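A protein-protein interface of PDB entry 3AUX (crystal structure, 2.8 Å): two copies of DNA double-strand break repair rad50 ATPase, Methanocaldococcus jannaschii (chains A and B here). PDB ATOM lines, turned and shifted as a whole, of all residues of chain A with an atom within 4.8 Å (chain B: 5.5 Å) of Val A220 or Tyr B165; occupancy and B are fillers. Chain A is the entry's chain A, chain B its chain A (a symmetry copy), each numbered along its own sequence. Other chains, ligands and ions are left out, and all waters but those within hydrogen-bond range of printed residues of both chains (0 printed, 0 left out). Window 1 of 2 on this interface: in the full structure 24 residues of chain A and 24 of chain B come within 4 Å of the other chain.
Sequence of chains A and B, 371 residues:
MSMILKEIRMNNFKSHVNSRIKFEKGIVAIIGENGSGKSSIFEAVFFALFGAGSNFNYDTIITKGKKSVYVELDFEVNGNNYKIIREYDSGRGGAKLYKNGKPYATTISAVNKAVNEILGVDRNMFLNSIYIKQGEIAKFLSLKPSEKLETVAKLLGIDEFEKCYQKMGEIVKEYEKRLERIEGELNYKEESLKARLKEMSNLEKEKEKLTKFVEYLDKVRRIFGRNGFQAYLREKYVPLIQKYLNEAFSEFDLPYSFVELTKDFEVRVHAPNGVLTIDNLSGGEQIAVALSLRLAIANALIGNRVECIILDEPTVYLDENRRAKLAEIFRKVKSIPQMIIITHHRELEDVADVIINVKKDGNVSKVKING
The side-chain hydroxyl (OH) of Tyr A165 is in hydrogen-bond range of the side-chain hydroxyl (OH) of Tyr B165 (3.0 Å).
The backbone NH (N) of Glu B162 lies within hydrogen-bond range of the side-chain hydroxyl (OH) of Tyr A216 (2.9 Å).
The backbone carbonyl oxygen of Glu B162 lies within hydrogen-bond range of the guanidinium group of Arg B221 (2.7 Å).
Among the printed residues, merely in contact across the chains: Leu A217 with Met B168 (3.6 Å), Ile A223 with Phe B229 (3.9 Å), Val A220 with Tyr B165 (3.99 Å) and Tyr A165 with Val B220 (3.99 Å).
Printed residues of chain B within 4 Å of Val A220: Tyr B165 (3.99 Å).
Of the printed residues of chain A, Tyr B165 touches Tyr A165 (3.0 Å) and Val A220 (3.99 Å).
Of the printed residues of chain B, Ile A223 touches Phe B229.
Printed residues of chain B within 4 Å of Tyr A165: Tyr B165 and Val B220.
Glu B170 touches none of the printed residues of chain A.
The nearest printed residue of chain B that does not touch Val A220 is Glu B162 (4.7 Å).
The nearest printed residue of chain B that does not touch Tyr A165 is Leu B217 (4.5 Å).
Of the 11 printed residues of chain A, 5 touch a printed residue of chain B.
Printed residues of chain A that touch a printed residue of chain B: Tyr A165, Tyr A216, Leu A217, Val A220 and Ile A223.
Hydrophobic or aromatic side chains of chain A within 4 Å of the printed part of chain B: Tyr A165, Tyr A216, Leu A217, Val A220 and Ile A223.
Of the 13 printed residues of chain B, 5 touch a printed residue of chain A.
Hydrophobic or aromatic side chains of chain B that line the printed part of chain A: Tyr B165, Met B168, Val B220 and Phe B229.
Tyr A165 touches its own counterpart, Tyr B165.
Tyr A165 touches Val B220, and with the chains exchanged Val A220 touches Tyr B165.
Positions printed for both chains: 165, 217, 220 and 221.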
ATOM      1  N   TYR A 165     -15.189   8.144  28.354  1.00  0.00           N
ATOM      2  CA  TYR A 165     -14.277   7.130  28.863  1.00  0.00           C
ATOM      3  C   TYR A 165     -14.802   6.555  30.157  1.00  0.00           C
ATOM      4  O   TYR A 165     -14.378   5.486  30.590  1.00  0.00           O
ATOM      5  CB  TYR A 165     -12.897   7.721  29.081  1.00  0.00           C
ATOM      6  CG  TYR A 165     -12.122   7.805  27.804  1.00  0.00           C
ATOM      7  CD1 TYR A 165     -11.586   6.661  27.222  1.00  0.00           C
ATOM      8  CD2 TYR A 165     -11.955   9.020  27.150  1.00  0.00           C
ATOM      9  CE1 TYR A 165     -10.903   6.724  26.021  1.00  0.00           C
ATOM     10  CE2 TYR A 165     -11.274   9.097  25.949  1.00  0.00           C
ATOM     11  CZ  TYR A 165     -10.752   7.946  25.390  1.00  0.00           C
ATOM     12  OH  TYR A 165     -10.072   8.024  24.201  1.00  0.00           O
ATOM     13  N   GLU A 215      -5.211   0.559  30.516  1.00  0.00           N
ATOM     14  CA  GLU A 215      -4.213   1.483  31.023  1.00  0.00           C
ATOM     15  C   GLU A 215      -4.006   2.585  30.001  1.00  0.00           C
ATOM     16  O   GLU A 215      -4.054   3.767  30.342  1.00  0.00           O
ATOM     17  CB  GLU A 215      -2.889   0.767  31.265  1.00  0.00           C
ATOM     18  CG  GLU A 215      -2.925  -0.231  32.393  1.00  0.00           C
ATOM     19  CD  GLU A 215      -1.564  -0.831  32.660  1.00  0.00           C
ATOM     20  OE1 GLU A 215      -1.015  -1.484  31.747  1.00  0.00           O
ATOM     21  OE2 GLU A 215      -1.042  -0.644  33.779  1.00  0.00           O
ATOM     22  N   TYR A 216      -3.780   2.200  28.747  1.00  0.00           N
ATOM     23  CA  TYR A 216      -3.571   3.192  27.704  1.00  0.00           C
ATOM     24  C   TYR A 216      -4.801   4.085  27.625  1.00  0.00           C
ATOM     25  O   TYR A 216      -4.757   5.156  27.024  1.00  0.00           O
ATOM     26  CB  TYR A 216      -3.310   2.541  26.341  1.00  0.00           C
ATOM     27  CG  TYR A 216      -2.540   3.458  25.410  1.00  0.00           C
ATOM     28  CD1 TYR A 216      -1.168   3.661  25.581  1.00  0.00           C
ATOM     29  CD2 TYR A 216      -3.190   4.182  24.408  1.00  0.00           C
ATOM     30  CE1 TYR A 216      -0.463   4.566  24.783  1.00  0.00           C
ATOM     31  CE2 TYR A 216      -2.495   5.093  23.603  1.00  0.00           C
ATOM     32  CZ  TYR A 216      -1.132   5.279  23.799  1.00  0.00           C
ATOM     33  OH  TYR A 216      -0.441   6.181  23.019  1.00  0.00           O
ATOM     34  N   LEU A 217      -5.899   3.640  28.232  1.00  0.00           N
ATOM     35  CA  LEU A 217      -7.126   4.427  28.254  1.00  0.00           C
ATOM     36  C   LEU A 217      -7.003   5.489  29.340  1.00  0.00           C
ATOM     37  O   LEU A 217      -7.442   6.626  29.170  1.00  0.00           O
ATOM     38  CB  LEU A 217      -8.345   3.546  28.533  1.00  0.00           C
ATOM     39  CG  LEU A 217      -8.925   2.750  27.364  1.00  0.00           C
ATOM     40  CD1 LEU A 217     -10.199   2.053  27.819  1.00  0.00           C
ATOM     41  CD2 LEU A 217      -9.226   3.679  26.200  1.00  0.00           C
ATOM     42  N   ASP A 218      -6.411   5.109  30.466  1.00  0.00           N
ATOM     43  CA  ASP A 218      -6.214   6.060  31.543  1.00  0.00           C
ATOM     44  C   ASP A 218      -5.073   6.987  31.162  1.00  0.00           C
ATOM     45  O   ASP A 218      -5.241   8.200  31.144  1.00  0.00           O
ATOM     46  CB  ASP A 218      -5.894   5.342  32.850  1.00  0.00           C
ATOM     47  CG  ASP A 218      -7.138   4.965  33.623  1.00  0.00           C
ATOM     48  OD1 ASP A 218      -7.899   5.877  34.010  1.00  0.00           O
ATOM     49  OD2 ASP A 218      -7.353   3.759  33.843  1.00  0.00           O
ATOM     50  N   LYS A 219      -3.919   6.412  30.838  1.00  0.00           N
ATOM     51  CA  LYS A 219      -2.754   7.202  30.452  1.00  0.00           C
ATOM     52  C   LYS A 219      -3.162   8.323  29.508  1.00  0.00           C
ATOM     53  O   LYS A 219      -2.533   9.378  29.479  1.00  0.00           O
ATOM     54  CB  LYS A 219      -1.704   6.310  29.786  1.00  0.00           C
ATOM     55  CG  LYS A 219      -1.197   5.185  30.688  1.00  0.00           C
ATOM     56  CD  LYS A 219      -0.186   4.282  29.984  1.00  0.00           C
ATOM     57  CE  LYS A 219       0.268   3.142  30.892  1.00  0.00           C
ATOM     58  NZ  LYS A 219       1.244   2.236  30.222  1.00  0.00           N
ATOM     59  N   VAL A 220      -4.226   8.092  28.742  1.00  0.00           N
ATOM     60  CA  VAL A 220      -4.737   9.084  27.800  1.00  0.00           C
ATOM     61  C   VAL A 220      -5.699  10.044  28.493  1.00  0.00           C
ATOM     62  O   VAL A 220      -5.456  11.250  28.541  1.00  0.00           O
ATOM     63  CB  VAL A 220      -5.466   8.410  26.611  1.00  0.00           C
ATOM     64  CG1 VAL A 220      -6.286   9.436  25.847  1.00  0.00           C
ATOM     65  CG2 VAL A 220      -4.449   7.762  25.680  1.00  0.00           C
ATOM     66  N   ARG A 221      -6.792   9.510  29.027  1.00  0.00           N
ATOM     67  CA  ARG A 221      -7.769  10.336  29.720  1.00  0.00           C
ATOM     68  C   ARG A 221      -7.101  11.110  30.850  1.00  0.00           C
ATOM     69  O   ARG A 221      -7.605  12.137  31.302  1.00  0.00           O
ATOM     70  CB  ARG A 221      -8.885   9.465  30.301  1.00  0.00           C
ATOM     71  CG  ARG A 221      -9.837  10.252  31.182  1.00  0.00           C
ATOM     72  CD  ARG A 221     -11.062   9.468  31.610  1.00  0.00           C
ATOM     73  NE  ARG A 221     -12.024  10.363  32.248  1.00  0.00           N
ATOM     74  CZ  ARG A 221     -12.597  11.403  31.642  1.00  0.00           C
ATOM     75  NH1 ARG A 221     -13.455  12.170  32.299  1.00  0.00           N
ATOM     76  NH2 ARG A 221     -12.326  11.676  30.374  1.00  0.00           N
ATOM     77  N   ARG A 222      -5.951  10.605  31.281  1.00  0.00           N
ATOM     78  CA  ARG A 222      -5.178  11.176  32.379  1.00  0.00           C
ATOM     79  C   ARG A 222      -4.301  12.375  31.989  1.00  0.00           C
ATOM     80  O   ARG A 222      -3.738  13.040  32.859  1.00  0.00           O
ATOM     81  CB  ARG A 222      -4.311  10.068  32.992  1.00  0.00           C
ATOM     82  CG  ARG A 222      -3.731  10.363  34.361  1.00  0.00           C
ATOM     83  CD  ARG A 222      -2.851   9.209  34.851  1.00  0.00           C
ATOM     84  NE  ARG A 222      -3.591   7.966  35.076  1.00  0.00           N
ATOM     85  CZ  ARG A 222      -4.597   7.832  35.938  1.00  0.00           C
ATOM     86  NH1 ARG A 222      -5.005   8.863  36.666  1.00  0.00           N
ATOM     87  NH2 ARG A 222      -5.193   6.657  36.080  1.00  0.00           N
ATOM     88  N   ILE A 223      -4.190  12.658  30.694  1.00  0.00           N
ATOM     89  CA  ILE A 223      -3.370  13.778  30.236  1.00  0.00           C
ATOM     90  C   ILE A 223      -4.193  14.950  29.705  1.00  0.00           C
ATOM     91  O   ILE A 223      -3.664  16.034  29.472  1.00  0.00           O
ATOM     92  CB  ILE A 223      -2.378  13.321  29.143  1.00  0.00           C
ATOM     93  CG1 ILE A 223      -1.411  12.292  29.728  1.00  0.00           C
ATOM     94  CG2 ILE A 223      -1.598  14.510  28.602  1.00  0.00           C
ATOM     95  CD1 ILE A 223      -0.337  11.844  28.767  1.00  0.00           C
ATOM     96  N   PHE A 224      -5.491  14.736  29.530  1.00  0.00           N
ATOM     97  CA  PHE A 224      -6.374  15.781  29.024  1.00  0.00           C
ATOM     98  C   PHE A 224      -7.097  16.533  30.128  1.00  0.00           C
ATOM     99  O   PHE A 224      -7.014  17.760  30.206  1.00  0.00           O
ATOM    100  CB  PHE A 224      -7.395  15.178  28.065  1.00  0.00           C
ATOM    101  CG  PHE A 224      -6.809  14.736  26.764  1.00  0.00           C
ATOM    102  CD1 PHE A 224      -6.346  15.672  25.848  1.00  0.00           C
ATOM    103  CD2 PHE A 224      -6.690  13.387  26.466  1.00  0.00           C
ATOM    104  CE1 PHE A 224      -5.783  15.272  24.649  1.00  0.00           C
ATOM    105  CE2 PHE A 224      -6.129  12.975  25.268  1.00  0.00           C
ATOM    106  CZ  PHE A 224      -5.668  13.918  24.359  1.00  0.00           C
ATOM    107  N   GLU B 162      -0.273   6.133  20.131  1.00  0.00           N
ATOM    108  CA  GLU B 162      -1.637   5.683  20.367  1.00  0.00           C
ATOM    109  C   GLU B 162      -2.140   4.689  19.322  1.00  0.00           C
ATOM    110  O   GLU B 162      -3.350   4.529  19.149  1.00  0.00           O
ATOM    111  CB  GLU B 162      -2.567   6.897  20.433  1.00  0.00           C
ATOM    112  CG  GLU B 162      -2.046   8.017  21.325  1.00  0.00           C
ATOM    113  CD  GLU B 162      -3.004   9.185  21.432  1.00  0.00           C
ATOM    114  OE1 GLU B 162      -2.624  10.203  22.039  1.00  0.00           O
ATOM    115  OE2 GLU B 162      -4.135   9.093  20.918  1.00  0.00           O
ATOM    116  N   LYS B 163      -1.218   4.025  18.626  1.00  0.00           N
ATOM    117  CA  LYS B 163      -1.594   3.028  17.625  1.00  0.00           C
ATOM    118  C   LYS B 163      -2.283   1.859  18.318  1.00  0.00           C
ATOM    119  O   LYS B 163      -2.855   0.991  17.663  1.00  0.00           O
ATOM    120  CB  LYS B 163      -0.366   2.504  16.874  1.00  0.00           C
ATOM    121  CG  LYS B 163       0.176   3.423  15.789  1.00  0.00           C
ATOM    122  CD  LYS B 163       1.300   2.732  15.013  1.00  0.00           C
ATOM    123  CE  LYS B 163       1.840   3.599  13.881  1.00  0.00           C
ATOM    124  NZ  LYS B 163       2.968   2.938  13.156  1.00  0.00           N
ATOM    125  N   CYS B 164      -2.209   1.838  19.648  1.00  0.00           N
ATOM    126  CA  CYS B 164      -2.834   0.783  20.434  1.00  0.00           C
ATOM    127  C   CYS B 164      -4.303   0.703  20.059  1.00  0.00           C
ATOM    128  O   CYS B 164      -4.906  -0.368  20.100  1.00  0.00           O
ATOM    129  CB  CYS B 164      -2.709   1.077  21.930  1.00  0.00           C
ATOM    130  SG  CYS B 164      -1.025   0.995  22.589  1.00  0.00           S
ATOM    131  N   TYR B 165      -4.873   1.849  19.694  1.00  0.00           N
ATOM    132  CA  TYR B 165      -6.271   1.914  19.295  1.00  0.00           C
ATOM    133  C   TYR B 165      -6.544   0.931  18.183  1.00  0.00           C
ATOM    134  O   TYR B 165      -7.694   0.585  17.914  1.00  0.00           O
ATOM    135  CB  TYR B 165      -6.629   3.318  18.846  1.00  0.00           C
ATOM    136  CG  TYR B 165      -6.898   4.221  20.008  1.00  0.00           C
ATOM    137  CD1 TYR B 165      -8.078   4.109  20.736  1.00  0.00           C
ATOM    138  CD2 TYR B 165      -5.959   5.163  20.411  1.00  0.00           C
ATOM    139  CE1 TYR B 165      -8.317   4.912  21.836  1.00  0.00           C
ATOM    140  CE2 TYR B 165      -6.186   5.972  21.510  1.00  0.00           C
ATOM    141  CZ  TYR B 165      -7.365   5.841  22.217  1.00  0.00           C
ATOM    142  OH  TYR B 165      -7.592   6.649  23.304  1.00  0.00           O
ATOM    143  N   GLN B 166      -5.475   0.489  17.535  1.00  0.00           N
ATOM    144  CA  GLN B 166      -5.590  -0.485  16.467  1.00  0.00           C
ATOM    145  C   GLN B 166      -6.363  -1.636  17.102  1.00  0.00           C
ATOM    146  O   GLN B 166      -7.534  -1.866  16.791  1.00  0.00           O
ATOM    147  CB  GLN B 166      -4.201  -0.962  16.035  1.00  0.00           C
ATOM    148  CG  GLN B 166      -4.129  -1.491  14.609  1.00  0.00           C
ATOM    149  CD  GLN B 166      -2.792  -2.133  14.293  1.00  0.00           C
ATOM    150  OE1 GLN B 166      -1.737  -1.616  14.669  1.00  0.00           O
ATOM    151  NE2 GLN B 166      -2.827  -3.261  13.591  1.00  0.00           N
ATOM    152  N   LYS B 167      -5.697  -2.335  18.018  1.00  0.00           N
ATOM    153  CA  LYS B 167      -6.294  -3.461  18.726  1.00  0.00           C
ATOM    154  C   LYS B 167      -7.547  -2.972  19.445  1.00  0.00           C
ATOM    155  O   LYS B 167      -8.545  -3.681  19.537  1.00  0.00           O
ATOM    156  CB  LYS B 167      -5.296  -4.024  19.742  1.00  0.00           C
ATOM    157  CG  LYS B 167      -3.894  -4.234  19.185  1.00  0.00           C
ATOM    158  CD  LYS B 167      -2.864  -3.491  20.018  1.00  0.00           C
ATOM    159  CE  LYS B 167      -1.468  -3.666  19.461  1.00  0.00           C
ATOM    160  NZ  LYS B 167      -0.457  -3.033  20.346  1.00  0.00           N
ATOM    161  N   MET B 168      -7.479  -1.742  19.938  1.00  0.00           N
ATOM    162  CA  MET B 168      -8.581  -1.127  20.663  1.00  0.00           C
ATOM    163  C   MET B 168      -9.875  -1.036  19.867  1.00  0.00           C
ATOM    164  O   MET B 168     -10.817  -1.788  20.111  1.00  0.00           O
ATOM    165  CB  MET B 168      -8.172   0.271  21.119  1.00  0.00           C
ATOM    166  CG  MET B 168      -7.966   0.390  22.606  1.00  0.00           C
ATOM    167  SD  MET B 168      -9.514   0.117  23.473  1.00  0.00           S
ATOM    168  CE  MET B 168     -10.242   1.763  23.383  1.00  0.00           C
ATOM    169  N   GLY B 169      -9.916  -0.101  18.925  1.00  0.00           N
ATOM    170  CA  GLY B 169     -11.102   0.088  18.114  1.00  0.00           C
ATOM    171  C   GLY B 169     -11.533  -1.138  17.332  1.00  0.00           C
ATOM    172  O   GLY B 169     -12.633  -1.160  16.787  1.00  0.00           O
ATOM    173  N   GLU B 170     -10.682  -2.157  17.280  1.00  0.00           N
ATOM    174  CA  GLU B 170     -11.012  -3.372  16.542  1.00  0.00           C
ATOM    175  C   GLU B 170     -11.524  -4.531  17.408  1.00  0.00           C
ATOM    176  O   GLU B 170     -12.591  -5.083  17.129  1.00  0.00           O
ATOM    177  CB  GLU B 170      -9.807  -3.815  15.700  1.00  0.00           C
ATOM    178  CG  GLU B 170      -9.510  -2.869  14.532  1.00  0.00           C
ATOM    179  CD  GLU B 170      -8.370  -3.341  13.636  1.00  0.00           C
ATOM    180  OE1 GLU B 170      -8.445  -4.476  13.115  1.00  0.00           O
ATOM    181  OE2 GLU B 170      -7.404  -2.571  13.444  1.00  0.00           O
ATOM    182  N   LEU B 217     -13.945   6.779  19.767  1.00  0.00           N
ATOM    183  CA  LEU B 217     -12.592   6.237  19.716  1.00  0.00           C
ATOM    184  C   LEU B 217     -11.914   6.739  18.449  1.00  0.00           C
ATOM    185  O   LEU B 217     -10.726   7.063  18.449  1.00  0.00           O
ATOM    186  CB  LEU B 217     -12.609   4.707  19.717  1.00  0.00           C
ATOM    187  CG  LEU B 217     -12.798   4.002  21.061  1.00  0.00           C
ATOM    188  CD1 LEU B 217     -12.651   2.501  20.861  1.00  0.00           C
ATOM    189  CD2 LEU B 217     -11.766   4.500  22.060  1.00  0.00           C
ATOM    190  N   VAL B 220     -11.400  10.555  18.301  1.00  0.00           N
ATOM    191  CA  VAL B 220     -10.215  10.879  19.089  1.00  0.00           C
ATOM    192  C   VAL B 220      -8.942  10.525  18.326  1.00  0.00           C
ATOM    193  O   VAL B 220      -8.122  11.395  18.037  1.00  0.00           O
ATOM    194  CB  VAL B 220     -10.216  10.127  20.443  1.00  0.00           C
ATOM    195  CG1 VAL B 220      -8.838  10.191  21.081  1.00  0.00           C
ATOM    196  CG2 VAL B 220     -11.249  10.746  21.377  1.00  0.00           C
ATOM    197  N   ARG B 221      -8.779   9.247  18.003  1.00  0.00           N
ATOM    198  CA  ARG B 221      -7.605   8.803  17.265  1.00  0.00           C
ATOM    199  C   ARG B 221      -7.482   9.573  15.955  1.00  0.00           C
ATOM    200  O   ARG B 221      -6.402   9.668  15.372  1.00  0.00           O
ATOM    201  CB  ARG B 221      -7.703   7.307  16.959  1.00  0.00           C
ATOM    202  CG  ARG B 221      -6.593   6.828  16.043  1.00  0.00           C
ATOM    203  CD  ARG B 221      -6.541   5.321  15.880  1.00  0.00           C
ATOM    204  NE  ARG B 221      -5.316   4.941  15.182  1.00  0.00           N
ATOM    205  CZ  ARG B 221      -4.086   5.181  15.640  1.00  0.00           C
ATOM    206  NH1 ARG B 221      -3.027   4.807  14.937  1.00  0.00           N
ATOM    207  NH2 ARG B 221      -3.909   5.784  16.806  1.00  0.00           N
ATOM    208  N   PHE B 229       0.143  14.402  19.157  1.00  0.00           N
ATOM    209  CA  PHE B 229       0.181  14.162  20.595  1.00  0.00           C
ATOM    210  C   PHE B 229       1.382  14.813  21.262  1.00  0.00           C
ATOM    211  O   PHE B 229       1.340  15.127  22.451  1.00  0.00           O
ATOM    212  CB  PHE B 229       0.197  12.665  20.878  1.00  0.00           C
ATOM    213  CG  PHE B 229      -0.140  12.321  22.293  1.00  0.00           C
ATOM    214  CD1 PHE B 229      -1.314  12.790  22.869  1.00  0.00           C
ATOM    215  CD2 PHE B 229       0.698  11.507  23.046  1.00  0.00           C
ATOM    216  CE1 PHE B 229      -1.651  12.450  24.177  1.00  0.00           C
ATOM    217  CE2 PHE B 229       0.370  11.160  24.359  1.00  0.00           C
ATOM    218  CZ  PHE B 229      -0.806  11.631  24.924  1.00  0.00           C
